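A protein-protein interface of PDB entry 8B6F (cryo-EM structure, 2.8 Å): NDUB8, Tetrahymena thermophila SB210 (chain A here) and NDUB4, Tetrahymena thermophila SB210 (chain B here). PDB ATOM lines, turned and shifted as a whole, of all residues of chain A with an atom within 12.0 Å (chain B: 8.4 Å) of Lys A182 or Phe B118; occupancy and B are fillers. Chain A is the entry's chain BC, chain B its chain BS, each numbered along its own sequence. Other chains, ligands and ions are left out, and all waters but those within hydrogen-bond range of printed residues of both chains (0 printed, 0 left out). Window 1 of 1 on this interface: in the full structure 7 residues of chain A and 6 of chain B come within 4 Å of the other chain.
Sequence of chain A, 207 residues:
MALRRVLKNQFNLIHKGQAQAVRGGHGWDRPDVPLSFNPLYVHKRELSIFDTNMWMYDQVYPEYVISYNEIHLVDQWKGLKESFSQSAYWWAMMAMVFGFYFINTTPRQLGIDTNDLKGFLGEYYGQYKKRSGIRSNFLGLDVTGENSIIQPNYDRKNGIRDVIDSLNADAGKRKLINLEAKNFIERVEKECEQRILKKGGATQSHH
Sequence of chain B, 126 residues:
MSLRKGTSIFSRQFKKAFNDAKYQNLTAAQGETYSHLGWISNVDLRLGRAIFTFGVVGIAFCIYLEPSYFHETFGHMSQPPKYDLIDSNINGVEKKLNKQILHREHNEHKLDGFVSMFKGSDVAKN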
ATOM      1  N   LYS A 173     -20.704 -10.343 -29.210  1.00  0.00           N
ATOM      2  CA  LYS A 173     -20.446  -9.593 -27.986  1.00  0.00           C
ATOM      3  C   LYS A 173     -19.123  -8.840 -28.068  1.00  0.00           C
ATOM      4  O   LYS A 173     -19.035  -7.682 -27.646  1.00  0.00           O
ATOM      5  CB  LYS A 173     -20.451 -10.539 -26.787  1.00  0.00           C
ATOM      6  CG  LYS A 173     -20.374  -9.837 -25.442  1.00  0.00           C
ATOM      7  CD  LYS A 173     -20.504 -10.827 -24.296  1.00  0.00           C
ATOM      8  CE  LYS A 173     -20.539 -10.113 -22.956  1.00  0.00           C
ATOM      9  NZ  LYS A 173     -20.686 -11.062 -21.820  1.00  0.00           N
ATOM     10  N   ARG A 174     -18.082  -9.479 -28.605  1.00  0.00           N
ATOM     11  CA  ARG A 174     -16.797  -8.799 -28.740  1.00  0.00           C
ATOM     12  C   ARG A 174     -16.892  -7.629 -29.712  1.00  0.00           C
ATOM     13  O   ARG A 174     -16.308  -6.567 -29.471  1.00  0.00           O
ATOM     14  CB  ARG A 174     -15.716  -9.789 -29.178  1.00  0.00           C
ATOM     15  CG  ARG A 174     -15.267 -10.709 -28.052  1.00  0.00           C
ATOM     16  CD  ARG A 174     -14.106 -11.608 -28.450  1.00  0.00           C
ATOM     17  NE  ARG A 174     -14.543 -12.772 -29.215  1.00  0.00           N
ATOM     18  CZ  ARG A 174     -14.240 -13.012 -30.485  1.00  0.00           C
ATOM     19  NH1 ARG A 174     -13.469 -12.195 -31.184  1.00  0.00           N
ATOM     20  NH2 ARG A 174     -14.724 -14.103 -31.069  1.00  0.00           N
ATOM     21  N   LYS A 175     -17.609  -7.806 -30.821  1.00  0.00           N
ATOM     22  CA  LYS A 175     -17.819  -6.695 -31.744  1.00  0.00           C
ATOM     23  C   LYS A 175     -18.573  -5.559 -31.064  1.00  0.00           C
ATOM     24  O   LYS A 175     -18.259  -4.382 -31.270  1.00  0.00           O
ATOM     25  CB  LYS A 175     -18.571  -7.171 -32.984  1.00  0.00           C
ATOM     26  CG  LYS A 175     -17.782  -8.145 -33.842  1.00  0.00           C
ATOM     27  CD  LYS A 175     -18.604  -8.672 -35.008  1.00  0.00           C
ATOM     28  CE  LYS A 175     -18.921  -7.575 -36.011  1.00  0.00           C
ATOM     29  NZ  LYS A 175     -19.632  -8.110 -37.206  1.00  0.00           N
ATOM     30  N   LEU A 176     -19.578  -5.895 -30.252  1.00  0.00           N
ATOM     31  CA  LEU A 176     -20.315  -4.869 -29.524  1.00  0.00           C
ATOM     32  C   LEU A 176     -19.406  -4.128 -28.553  1.00  0.00           C
ATOM     33  O   LEU A 176     -19.506  -2.905 -28.409  1.00  0.00           O
ATOM     34  CB  LEU A 176     -21.493  -5.500 -28.780  1.00  0.00           C
ATOM     35  CG  LEU A 176     -22.385  -4.547 -27.979  1.00  0.00           C
ATOM     36  CD1 LEU A 176     -23.075  -3.548 -28.894  1.00  0.00           C
ATOM     37  CD2 LEU A 176     -23.407  -5.331 -27.176  1.00  0.00           C
ATOM     38  N   ILE A 177     -18.513  -4.853 -27.879  1.00  0.00           N
ATOM     39  CA  ILE A 177     -17.577  -4.210 -26.962  1.00  0.00           C
ATOM     40  C   ILE A 177     -16.681  -3.235 -27.713  1.00  0.00           C
ATOM     41  O   ILE A 177     -16.438  -2.113 -27.253  1.00  0.00           O
ATOM     42  CB  ILE A 177     -16.757  -5.277 -26.211  1.00  0.00           C
ATOM     43  CG1 ILE A 177     -17.659  -6.047 -25.243  1.00  0.00           C
ATOM     44  CG2 ILE A 177     -15.588  -4.643 -25.466  1.00  0.00           C
ATOM     45  CD1 ILE A 177     -17.030  -7.303 -24.686  1.00  0.00           C
ATOM     46  N   ASN A 178     -16.166  -3.645 -28.871  1.00  0.00           N
ATOM     47  CA  ASN A 178     -15.336  -2.744 -29.663  1.00  0.00           C
ATOM     48  C   ASN A 178     -16.119  -1.510 -30.091  1.00  0.00           C
ATOM     49  O   ASN A 178     -15.606  -0.388 -30.026  1.00  0.00           O
ATOM     50  CB  ASN A 178     -14.788  -3.477 -30.886  1.00  0.00           C
ATOM     51  CG  ASN A 178     -13.808  -4.572 -30.520  1.00  0.00           C
ATOM     52  OD1 ASN A 178     -13.085  -4.471 -29.532  1.00  0.00           O
ATOM     53  ND2 ASN A 178     -13.784  -5.631 -31.318  1.00  0.00           N
ATOM     54  N   LEU A 179     -17.365  -1.697 -30.533  1.00  0.00           N
ATOM     55  CA  LEU A 179     -18.178  -0.560 -30.949  1.00  0.00           C
ATOM     56  C   LEU A 179     -18.439   0.388 -29.785  1.00  0.00           C
ATOM     57  O   LEU A 179     -18.402   1.612 -29.949  1.00  0.00           O
ATOM     58  CB  LEU A 179     -19.497  -1.052 -31.546  1.00  0.00           C
ATOM     59  CG  LEU A 179     -20.472   0.031 -32.014  1.00  0.00           C
ATOM     60  CD1 LEU A 179     -19.840   0.923 -33.068  1.00  0.00           C
ATOM     61  CD2 LEU A 179     -21.744  -0.602 -32.546  1.00  0.00           C
ATOM     62  N   GLU A 180     -18.709  -0.161 -28.599  1.00  0.00           N
ATOM     63  CA  GLU A 180     -18.931   0.679 -27.428  1.00  0.00           C
ATOM     64  C   GLU A 180     -17.675   1.455 -27.060  1.00  0.00           C
ATOM     65  O   GLU A 180     -17.751   2.623 -26.663  1.00  0.00           O
ATOM     66  CB  GLU A 180     -19.400  -0.176 -26.252  1.00  0.00           C
ATOM     67  CG  GLU A 180     -20.808  -0.720 -26.420  1.00  0.00           C
ATOM     68  CD  GLU A 180     -21.231  -1.607 -25.268  1.00  0.00           C
ATOM     69  OE1 GLU A 180     -20.396  -1.860 -24.376  1.00  0.00           O
ATOM     70  OE2 GLU A 180     -22.396  -2.053 -25.253  1.00  0.00           O
ATOM     71  N   ALA A 181     -16.506   0.822 -27.177  1.00  0.00           N
ATOM     72  CA  ALA A 181     -15.261   1.536 -26.922  1.00  0.00           C
ATOM     73  C   ALA A 181     -15.076   2.677 -27.911  1.00  0.00           C
ATOM     74  O   ALA A 181     -14.660   3.778 -27.532  1.00  0.00           O
ATOM     75  CB  ALA A 181     -14.078   0.571 -26.990  1.00  0.00           C
ATOM     76  N   LYS A 182     -15.375   2.434 -29.188  1.00  0.00           N
ATOM     77  CA  LYS A 182     -15.283   3.497 -30.182  1.00  0.00           C
ATOM     78  C   LYS A 182     -16.233   4.638 -29.845  1.00  0.00           C
ATOM     79  O   LYS A 182     -15.862   5.813 -29.934  1.00  0.00           O
ATOM     80  CB  LYS A 182     -15.580   2.938 -31.573  1.00  0.00           C
ATOM     81  CG  LYS A 182     -15.599   3.988 -32.673  1.00  0.00           C
ATOM     82  CD  LYS A 182     -15.821   3.353 -34.034  1.00  0.00           C
ATOM     83  CE  LYS A 182     -15.835   4.402 -35.130  1.00  0.00           C
ATOM     84  NZ  LYS A 182     -15.999   3.793 -36.477  1.00  0.00           N
ATOM     85  N   ASN A 183     -17.467   4.311 -29.464  1.00  0.00           N
ATOM     86  CA  ASN A 183     -18.422   5.347 -29.083  1.00  0.00           C
ATOM     87  C   ASN A 183     -17.924   6.136 -27.880  1.00  0.00           C
ATOM     88  O   ASN A 183     -18.086   7.358 -27.818  1.00  0.00           O
ATOM     89  CB  ASN A 183     -19.785   4.725 -28.788  1.00  0.00           C
ATOM     90  CG  ASN A 183     -20.434   4.138 -30.022  1.00  0.00           C
ATOM     91  OD1 ASN A 183     -20.189   4.586 -31.140  1.00  0.00           O
ATOM     92  ND2 ASN A 183     -21.274   3.127 -29.825  1.00  0.00           N
ATOM     93  N   PHE A 184     -17.313   5.450 -26.911  1.00  0.00           N
ATOM     94  CA  PHE A 184     -16.782   6.144 -25.742  1.00  0.00           C
ATOM     95  C   PHE A 184     -15.684   7.127 -26.124  1.00  0.00           C
ATOM     96  O   PHE A 184     -15.669   8.263 -25.639  1.00  0.00           O
ATOM     97  CB  PHE A 184     -16.250   5.131 -24.730  1.00  0.00           C
ATOM     98  CG  PHE A 184     -15.189   5.685 -23.826  1.00  0.00           C
ATOM     99  CD1 PHE A 184     -15.527   6.497 -22.756  1.00  0.00           C
ATOM    100  CD2 PHE A 184     -13.853   5.392 -24.043  1.00  0.00           C
ATOM    101  CE1 PHE A 184     -14.553   7.009 -21.922  1.00  0.00           C
ATOM    102  CE2 PHE A 184     -12.873   5.901 -23.212  1.00  0.00           C
ATOM    103  CZ  PHE A 184     -13.225   6.710 -22.149  1.00  0.00           C
ATOM    104  N   ILE A 185     -14.761   6.719 -26.993  1.00  0.00           N
ATOM    105  CA  ILE A 185     -13.673   7.619 -27.363  1.00  0.00           C
ATOM    106  C   ILE A 185     -14.218   8.817 -28.129  1.00  0.00           C
ATOM    107  O   ILE A 185     -13.757   9.948 -27.947  1.00  0.00           O
ATOM    108  CB  ILE A 185     -12.590   6.861 -28.157  1.00  0.00           C
ATOM    109  CG1 ILE A 185     -11.203   7.436 -27.859  1.00  0.00           C
ATOM    110  CG2 ILE A 185     -12.835   6.921 -29.660  1.00  0.00           C
ATOM    111  CD1 ILE A 185     -10.708   7.177 -26.448  1.00  0.00           C
ATOM    112  N   GLU A 186     -15.200   8.590 -29.005  1.00  0.00           N
ATOM    113  CA  GLU A 186     -15.815   9.705 -29.716  1.00  0.00           C
ATOM    114  C   GLU A 186     -16.503  10.658 -28.747  1.00  0.00           C
ATOM    115  O   GLU A 186     -16.390  11.880 -28.880  1.00  0.00           O
ATOM    116  CB  GLU A 186     -16.812   9.183 -30.750  1.00  0.00           C
ATOM    117  CG  GLU A 186     -16.170   8.410 -31.888  1.00  0.00           C
ATOM    118  CD  GLU A 186     -17.191   7.859 -32.864  1.00  0.00           C
ATOM    119  OE1 GLU A 186     -18.403   8.040 -32.621  1.00  0.00           O
ATOM    120  OE2 GLU A 186     -16.781   7.249 -33.874  1.00  0.00           O
ATOM    121  N   ARG A 187     -17.220  10.114 -27.761  1.00  0.00           N
ATOM    122  CA  ARG A 187     -17.895  10.964 -26.788  1.00  0.00           C
ATOM    123  C   ARG A 187     -16.892  11.778 -25.981  1.00  0.00           C
ATOM    124  O   ARG A 187     -17.116  12.963 -25.713  1.00  0.00           O
ATOM    125  CB  ARG A 187     -18.758  10.114 -25.856  1.00  0.00           C
ATOM    126  CG  ARG A 187     -19.732  10.924 -25.016  1.00  0.00           C
ATOM    127  CD  ARG A 187     -20.325  10.103 -23.882  1.00  0.00           C
ATOM    128  NE  ARG A 187     -20.665   8.747 -24.297  1.00  0.00           N
ATOM    129  CZ  ARG A 187     -19.937   7.668 -24.038  1.00  0.00           C
ATOM    130  NH1 ARG A 187     -18.810   7.738 -23.349  1.00  0.00           N
ATOM    131  NH2 ARG A 187     -20.354   6.484 -24.479  1.00  0.00           N
ATOM    132  N   VAL A 188     -15.779  11.159 -25.584  1.00  0.00           N
ATOM    133  CA  VAL A 188     -14.759  11.886 -24.832  1.00  0.00           C
ATOM    134  C   VAL A 188     -14.179  13.012 -25.675  1.00  0.00           C
ATOM    135  O   VAL A 188     -13.980  14.131 -25.188  1.00  0.00           O
ATOM    136  CB  VAL A 188     -13.665  10.916 -24.346  1.00  0.00           C
ATOM    137  CG1 VAL A 188     -12.453  11.677 -23.820  1.00  0.00           C
ATOM    138  CG2 VAL A 188     -14.217   9.997 -23.271  1.00  0.00           C
ATOM    139  N   GLU A 189     -13.894  12.738 -26.949  1.00  0.00           N
ATOM    140  CA  GLU A 189     -13.371  13.784 -27.820  1.00  0.00           C
ATOM    141  C   GLU A 189     -14.360  14.935 -27.945  1.00  0.00           C
ATOM    142  O   GLU A 189     -13.974  16.106 -27.862  1.00  0.00           O
ATOM    143  CB  GLU A 189     -13.049  13.204 -29.197  1.00  0.00           C
ATOM    144  CG  GLU A 189     -12.436  14.207 -30.163  1.00  0.00           C
ATOM    145  CD  GLU A 189     -12.240  13.633 -31.550  1.00  0.00           C
ATOM    146  OE1 GLU A 189     -12.516  12.430 -31.740  1.00  0.00           O
ATOM    147  OE2 GLU A 189     -11.814  14.384 -32.453  1.00  0.00           O
ATOM    148  N   LYS A 190     -15.642  14.621 -28.144  1.00  0.00           N
ATOM    149  CA  LYS A 190     -16.645  15.673 -28.276  1.00  0.00           C
ATOM    150  C   LYS A 190     -16.764  16.484 -26.993  1.00  0.00           C
ATOM    151  O   LYS A 190     -16.863  17.716 -27.035  1.00  0.00           O
ATOM    152  CB  LYS A 190     -17.997  15.069 -28.654  1.00  0.00           C
ATOM    153  CG  LYS A 190     -18.023  14.392 -30.018  1.00  0.00           C
ATOM    154  CD  LYS A 190     -17.761  15.379 -31.145  1.00  0.00           C
ATOM    155  CE  LYS A 190     -17.890  14.712 -32.506  1.00  0.00           C
ATOM    156  NZ  LYS A 190     -16.956  13.561 -32.666  1.00  0.00           N
ATOM    157  N   GLU A 191     -16.755  15.814 -25.839  1.00  0.00           N
ATOM    158  CA  GLU A 191     -16.853  16.533 -24.573  1.00  0.00           C
ATOM    159  C   GLU A 191     -15.657  17.451 -24.366  1.00  0.00           C
ATOM    160  O   GLU A 191     -15.812  18.593 -23.918  1.00  0.00           O
ATOM    161  CB  GLU A 191     -16.975  15.542 -23.414  1.00  0.00           C
ATOM    162  CG  GLU A 191     -18.307  14.808 -23.371  1.00  0.00           C
ATOM    163  CD  GLU A 191     -18.381  13.798 -22.242  1.00  0.00           C
ATOM    164  OE1 GLU A 191     -17.436  13.746 -21.426  1.00  0.00           O
ATOM    165  OE2 GLU A 191     -19.383  13.055 -22.169  1.00  0.00           O
ATOM    166  N   LEU B 111      -1.084  10.087 -26.792  1.00  0.00           N
ATOM    167  CA  LEU B 111      -2.535  10.224 -26.830  1.00  0.00           C
ATOM    168  C   LEU B 111      -3.082   9.862 -28.203  1.00  0.00           C
ATOM    169  O   LEU B 111      -4.130   9.217 -28.313  1.00  0.00           O
ATOM    170  CB  LEU B 111      -2.959  11.640 -26.447  1.00  0.00           C
ATOM    171  CG  LEU B 111      -4.479  11.791 -26.541  1.00  0.00           C
ATOM    172  CD1 LEU B 111      -5.053  12.391 -25.294  1.00  0.00           C
ATOM    173  CD2 LEU B 111      -4.838  12.651 -27.744  1.00  0.00           C
ATOM    174  N   ASP B 112      -2.374  10.256 -29.264  1.00  0.00           N
ATOM    175  CA  ASP B 112      -2.830   9.941 -30.613  1.00  0.00           C
ATOM    176  C   ASP B 112      -2.851   8.439 -30.842  1.00  0.00           C
ATOM    177  O   ASP B 112      -3.787   7.909 -31.451  1.00  0.00           O
ATOM    178  CB  ASP B 112      -1.937  10.628 -31.645  1.00  0.00           C
ATOM    179  CG  ASP B 112      -2.068  12.137 -31.615  1.00  0.00           C
ATOM    180  OD1 ASP B 112      -2.877  12.647 -30.813  1.00  0.00           O
ATOM    181  OD2 ASP B 112      -1.362  12.815 -32.392  1.00  0.00           O
ATOM    182  N   GLY B 113      -1.826   7.733 -30.369  1.00  0.00           N
ATOM    183  CA  GLY B 113      -1.840   6.285 -30.483  1.00  0.00           C
ATOM    184  C   GLY B 113      -3.018   5.668 -29.756  1.00  0.00           C
ATOM    185  O   GLY B 113      -3.692   4.779 -30.281  1.00  0.00           O
ATOM    186  N   PHE B 114      -3.279   6.129 -28.531  1.00  0.00           N
ATOM    187  CA  PHE B 114      -4.396   5.594 -27.759  1.00  0.00           C
ATOM    188  C   PHE B 114      -5.723   5.825 -28.476  1.00  0.00           C
ATOM    189  O   PHE B 114      -6.526   4.898 -28.633  1.00  0.00           O
ATOM    190  CB  PHE B 114      -4.410   6.235 -26.371  1.00  0.00           C
ATOM    191  CG  PHE B 114      -5.514   5.743 -25.481  1.00  0.00           C
ATOM    192  CD1 PHE B 114      -5.440   4.492 -24.894  1.00  0.00           C
ATOM    193  CD2 PHE B 114      -6.618   6.536 -25.221  1.00  0.00           C
ATOM    194  CE1 PHE B 114      -6.448   4.037 -24.069  1.00  0.00           C
ATOM    195  CE2 PHE B 114      -7.632   6.086 -24.396  1.00  0.00           C
ATOM    196  CZ  PHE B 114      -7.545   4.834 -23.819  1.00  0.00           C
ATOM    197  N   VAL B 115      -5.972   7.058 -28.921  1.00  0.00           N
ATOM    198  CA  VAL B 115      -7.255   7.372 -29.544  1.00  0.00           C
ATOM    199  C   VAL B 115      -7.397   6.650 -30.878  1.00  0.00           C
ATOM    200  O   VAL B 115      -8.489   6.202 -31.244  1.00  0.00           O
ATOM    201  CB  VAL B 115      -7.429   8.895 -29.705  1.00  0.00           C
ATOM    202  CG1 VAL B 115      -7.378   9.583 -28.352  1.00  0.00           C
ATOM    203  CG2 VAL B 115      -6.381   9.465 -30.640  1.00  0.00           C
ATOM    204  N   SER B 116      -6.299   6.521 -31.625  1.00  0.00           N
ATOM    205  CA  SER B 116      -6.357   5.801 -32.892  1.00  0.00           C
ATOM    206  C   SER B 116      -6.682   4.332 -32.672  1.00  0.00           C
ATOM    207  O   SER B 116      -7.485   3.749 -33.410  1.00  0.00           O
ATOM    208  CB  SER B 116      -5.034   5.952 -33.643  1.00  0.00           C
ATOM    209  OG  SER B 116      -3.960   5.404 -32.899  1.00  0.00           O
ATOM    210  N   MET B 117      -6.064   3.711 -31.668  1.00  0.00           N
ATOM    211  CA  MET B 117      -6.391   2.323 -31.364  1.00  0.00           C
ATOM    212  C   MET B 117      -7.862   2.178 -30.999  1.00  0.00           C
ATOM    213  O   MET B 117      -8.525   1.227 -31.429  1.00  0.00           O
ATOM    214  CB  MET B 117      -5.502   1.820 -30.227  1.00  0.00           C
ATOM    215  CG  MET B 117      -5.816   0.406 -29.765  1.00  0.00           C
ATOM    216  SD  MET B 117      -5.713  -0.810 -31.089  1.00  0.00           S
ATOM    217  CE  MET B 117      -3.960  -0.778 -31.444  1.00  0.00           C
ATOM    218  N   PHE B 118      -8.391   3.110 -30.205  1.00  0.00           N
ATOM    219  CA  PHE B 118      -9.791   3.023 -29.800  1.00  0.00           C
ATOM    220  C   PHE B 118     -10.730   3.263 -30.978  1.00  0.00           C
ATOM    221  O   PHE B 118     -11.771   2.606 -31.090  1.00  0.00           O
ATOM    222  CB  PHE B 118     -10.073   4.015 -28.673  1.00  0.00           C
ATOM    223  CG  PHE B 118     -10.121   3.379 -27.314  1.00  0.00           C
ATOM    224  CD1 PHE B 118      -8.968   2.883 -26.729  1.00  0.00           C
ATOM    225  CD2 PHE B 118     -11.316   3.270 -26.626  1.00  0.00           C
ATOM    226  CE1 PHE B 118      -9.007   2.295 -25.481  1.00  0.00           C
ATOM    227  CE2 PHE B 118     -11.361   2.682 -25.378  1.00  0.00           C
ATOM    228  CZ  PHE B 118     -10.205   2.195 -24.805  1.00  0.00           C
ATOM    229  N   LYS B 119     -10.385   4.203 -31.860  1.00  0.00           N
ATOM    230  CA  LYS B 119     -11.293   4.570 -32.943  1.00  0.00           C
ATOM    231  C   LYS B 119     -11.292   3.543 -34.069  1.00  0.00           C
ATOM    232  O   LYS B 119     -12.342   3.270 -34.660  1.00  0.00           O
ATOM    233  CB  LYS B 119     -10.919   5.943 -33.503  1.00  0.00           C
ATOM    234  CG  LYS B 119     -11.210   7.104 -32.574  1.00  0.00           C
ATOM    235  CD  LYS B 119     -10.748   8.417 -33.184  1.00  0.00           C
ATOM    236  CE  LYS B 119     -11.020   9.583 -32.250  1.00  0.00           C
ATOM    237  NZ  LYS B 119     -10.485  10.862 -32.794  1.00  0.00           N
ATOM    238  N   GLY B 120     -10.135   2.966 -34.378  1.00  0.00           N
ATOM    239  CA  GLY B 120      -9.997   2.153 -35.572  1.00  0.00           C
ATOM    240  C   GLY B 120     -10.644   0.784 -35.500  1.00  0.00           C
ATOM    241  O   GLY B 120     -10.329  -0.089 -36.311  1.00  0.00           O
ATOM    242  N   SER B 121     -11.553   0.580 -34.545  1.00  0.00           N
ATOM    243  CA  SER B 121     -12.179  -0.729 -34.396  1.00  0.00           C
ATOM    244  C   SER B 121     -12.996  -1.108 -35.623  1.00  0.00           C
ATOM    245  O   SER B 121     -13.152  -2.299 -35.918  1.00  0.00           O
ATOM    246  CB  SER B 121     -13.058  -0.751 -33.148  1.00  0.00           C
ATOM    247  OG  SER B 121     -14.101   0.201 -33.240  1.00  0.00           O
ATOM    248  N   ASP B 122     -13.526  -0.122 -36.344  1.00  0.00           N
ATOM    249  CA  ASP B 122     -14.410  -0.360 -37.477  1.00  0.00           C
ATOM    250  C   ASP B 122     -13.703  -0.216 -38.820  1.00  0.00           C
ATOM    251  O   ASP B 122     -14.373  -0.163 -39.856  1.00  0.00           O
ATOM    252  CB  ASP B 122     -15.601   0.599 -37.412  1.00  0.00           C
ATOM    253  CG  ASP B 122     -16.740   0.181 -38.320  1.00  0.00           C
ATOM    254  OD1 ASP B 122     -16.657  -0.912 -38.919  1.00  0.00           O
ATOM    255  OD2 ASP B 122     -17.721   0.946 -38.439  1.00  0.00           O
ATOM    256  N   VAL B 123     -12.371  -0.152 -38.833  1.00  0.00           N
ATOM    257  CA  VAL B 123     -11.654   0.004 -40.097  1.00  0.00           C
ATOM    258  C   VAL B 123     -11.899  -1.198 -41.001  1.00  0.00           C
ATOM    259  O   VAL B 123     -12.118  -1.049 -42.209  1.00  0.00           O
ATOM    260  CB  VAL B 123     -10.152   0.224 -39.836  1.00  0.00           C
ATOM    261  CG1 VAL B 123      -9.351   0.123 -41.132  1.00  0.00           C
ATOM    262  CG2 VAL B 123      -9.926   1.573 -39.183  1.00  0.00           C
ATOM    263  N   LYS B 125     -14.054  -3.754 -42.594  1.00  0.00           N
ATOM    264  CA  LYS B 125     -15.467  -3.977 -42.874  1.00  0.00           C
ATOM    265  C   LYS B 125     -15.710  -5.427 -43.279  1.00  0.00           C
ATOM    266  O   LYS B 125     -16.790  -5.972 -43.051  1.00  0.00           O
ATOM    267  CB  LYS B 125     -15.951  -3.035 -43.979  1.00  0.00           C
ATOM    268  CG  LYS B 125     -15.774  -1.553 -43.665  1.00  0.00           C
ATOM    269  CD  LYS B 125     -16.567  -1.143 -42.433  1.00  0.00           C
ATOM    270  CE  LYS B 125     -16.488   0.358 -42.197  1.00  0.00           C
ATOM    271  NZ  LYS B 125     -15.084   0.834 -42.053  1.00  0.00           N
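The side-chain amino group (NZ) of Lys A182 is in salt-bridge range of the side-chain carboxylate (OD2) of Asp B122 (3.9 Å).
The side-chain carboxylate (OE1) of Glu A189 is in salt-bridge range of the side-chain amino group (NZ) of Lys B119 (2.8 Å).
The side-chain carboxylate (OD1) of Asp B122 is in salt-bridge range of the side-chain amino group (NZ) of Lys B125 (3.9 Å).
The side-chain amide nitrogen of Asn A178 lies within hydrogen-bond range of the backbone carbonyl oxygen of Arg A174 (3.3 Å).
Ser B121 touches Asn A178 (OG to O, 3.6 Å).
O of Ala A181 touches CD2 of Phe B118 (3.5 Å).
O of Phe B118 touches CA of Lys A182, 3.7 Å away.
CD of Lys A182 touches O of Lys B119, 3.5 Å away.
Ser B121 touches Lys A182.
Phe A184 touches Phe B118.
CE2 of Phe B114 touches CD1 of Ile A185 (3.9 Å).
Ile A185 touches Phe B118.
Ile A185 touches Lys B119 (CG2 to CG, 3.3 Å).
Printed residues of chain B within 4 Å of Lys A182: Phe B118, Lys B119, Ser B121 and Asp B122.
Printed residues of chain A within 4 Å of Phe B118: Ala A181, Lys A182, Phe A184 and Ile A185.
Printed residues of chain B within 4 Å of Ala A181: Phe B118 (3.5 Å).
Of chain A, only Ile A185 (3.9 Å) comes within 4 Å of Phe B114.
No residue of chain A comes within 4 Å of Val B115.
No residue of chain A comes within 4 Å of Ser B116.
No residue of chain A comes within 4 Å of Met B117.
Of chain A, only Asn A178 and Lys A182 come within 4 Å of Ser B121.
Printed residues of chain A within 4 Å of Asp B122: Lys A182 (3.4 Å).
Printed residues of chain B within 4 Å of Glu A189: Lys B119 (2.8 Å).
Printed residues of chain B within 4 Å of Ile A185: Phe B114 (3.9 Å), Phe B118 (3.7 Å) and Lys B119 (3.3 Å).
Of the printed residues of chain B, Phe A184 touches Phe B118.
The nearest residue of chain B that does not touch Lys A182 is Gly B120 (5.7 Å).
Of the 19 printed residues of chain A, 6 touch a printed residue of chain B.
Printed residues of chain A that touch a printed residue of chain B: Asn A178, Ala A181, Lys A182, Phe A184, Ile A185 and Glu A189.
Hydrophobic or aromatic side chains of chain A that line the printed part of chain B: Ala A181, Phe A184 and Ile A185.
Of the 14 printed residues of chain B, 5 touch a printed residue of chain A.
Hydrophobic or aromatic side chains of chain B within 4 Å of the printed part of chain A: Phe B114 and Phe B118.
Among the printed residues, 11 pairs touch across the chains.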
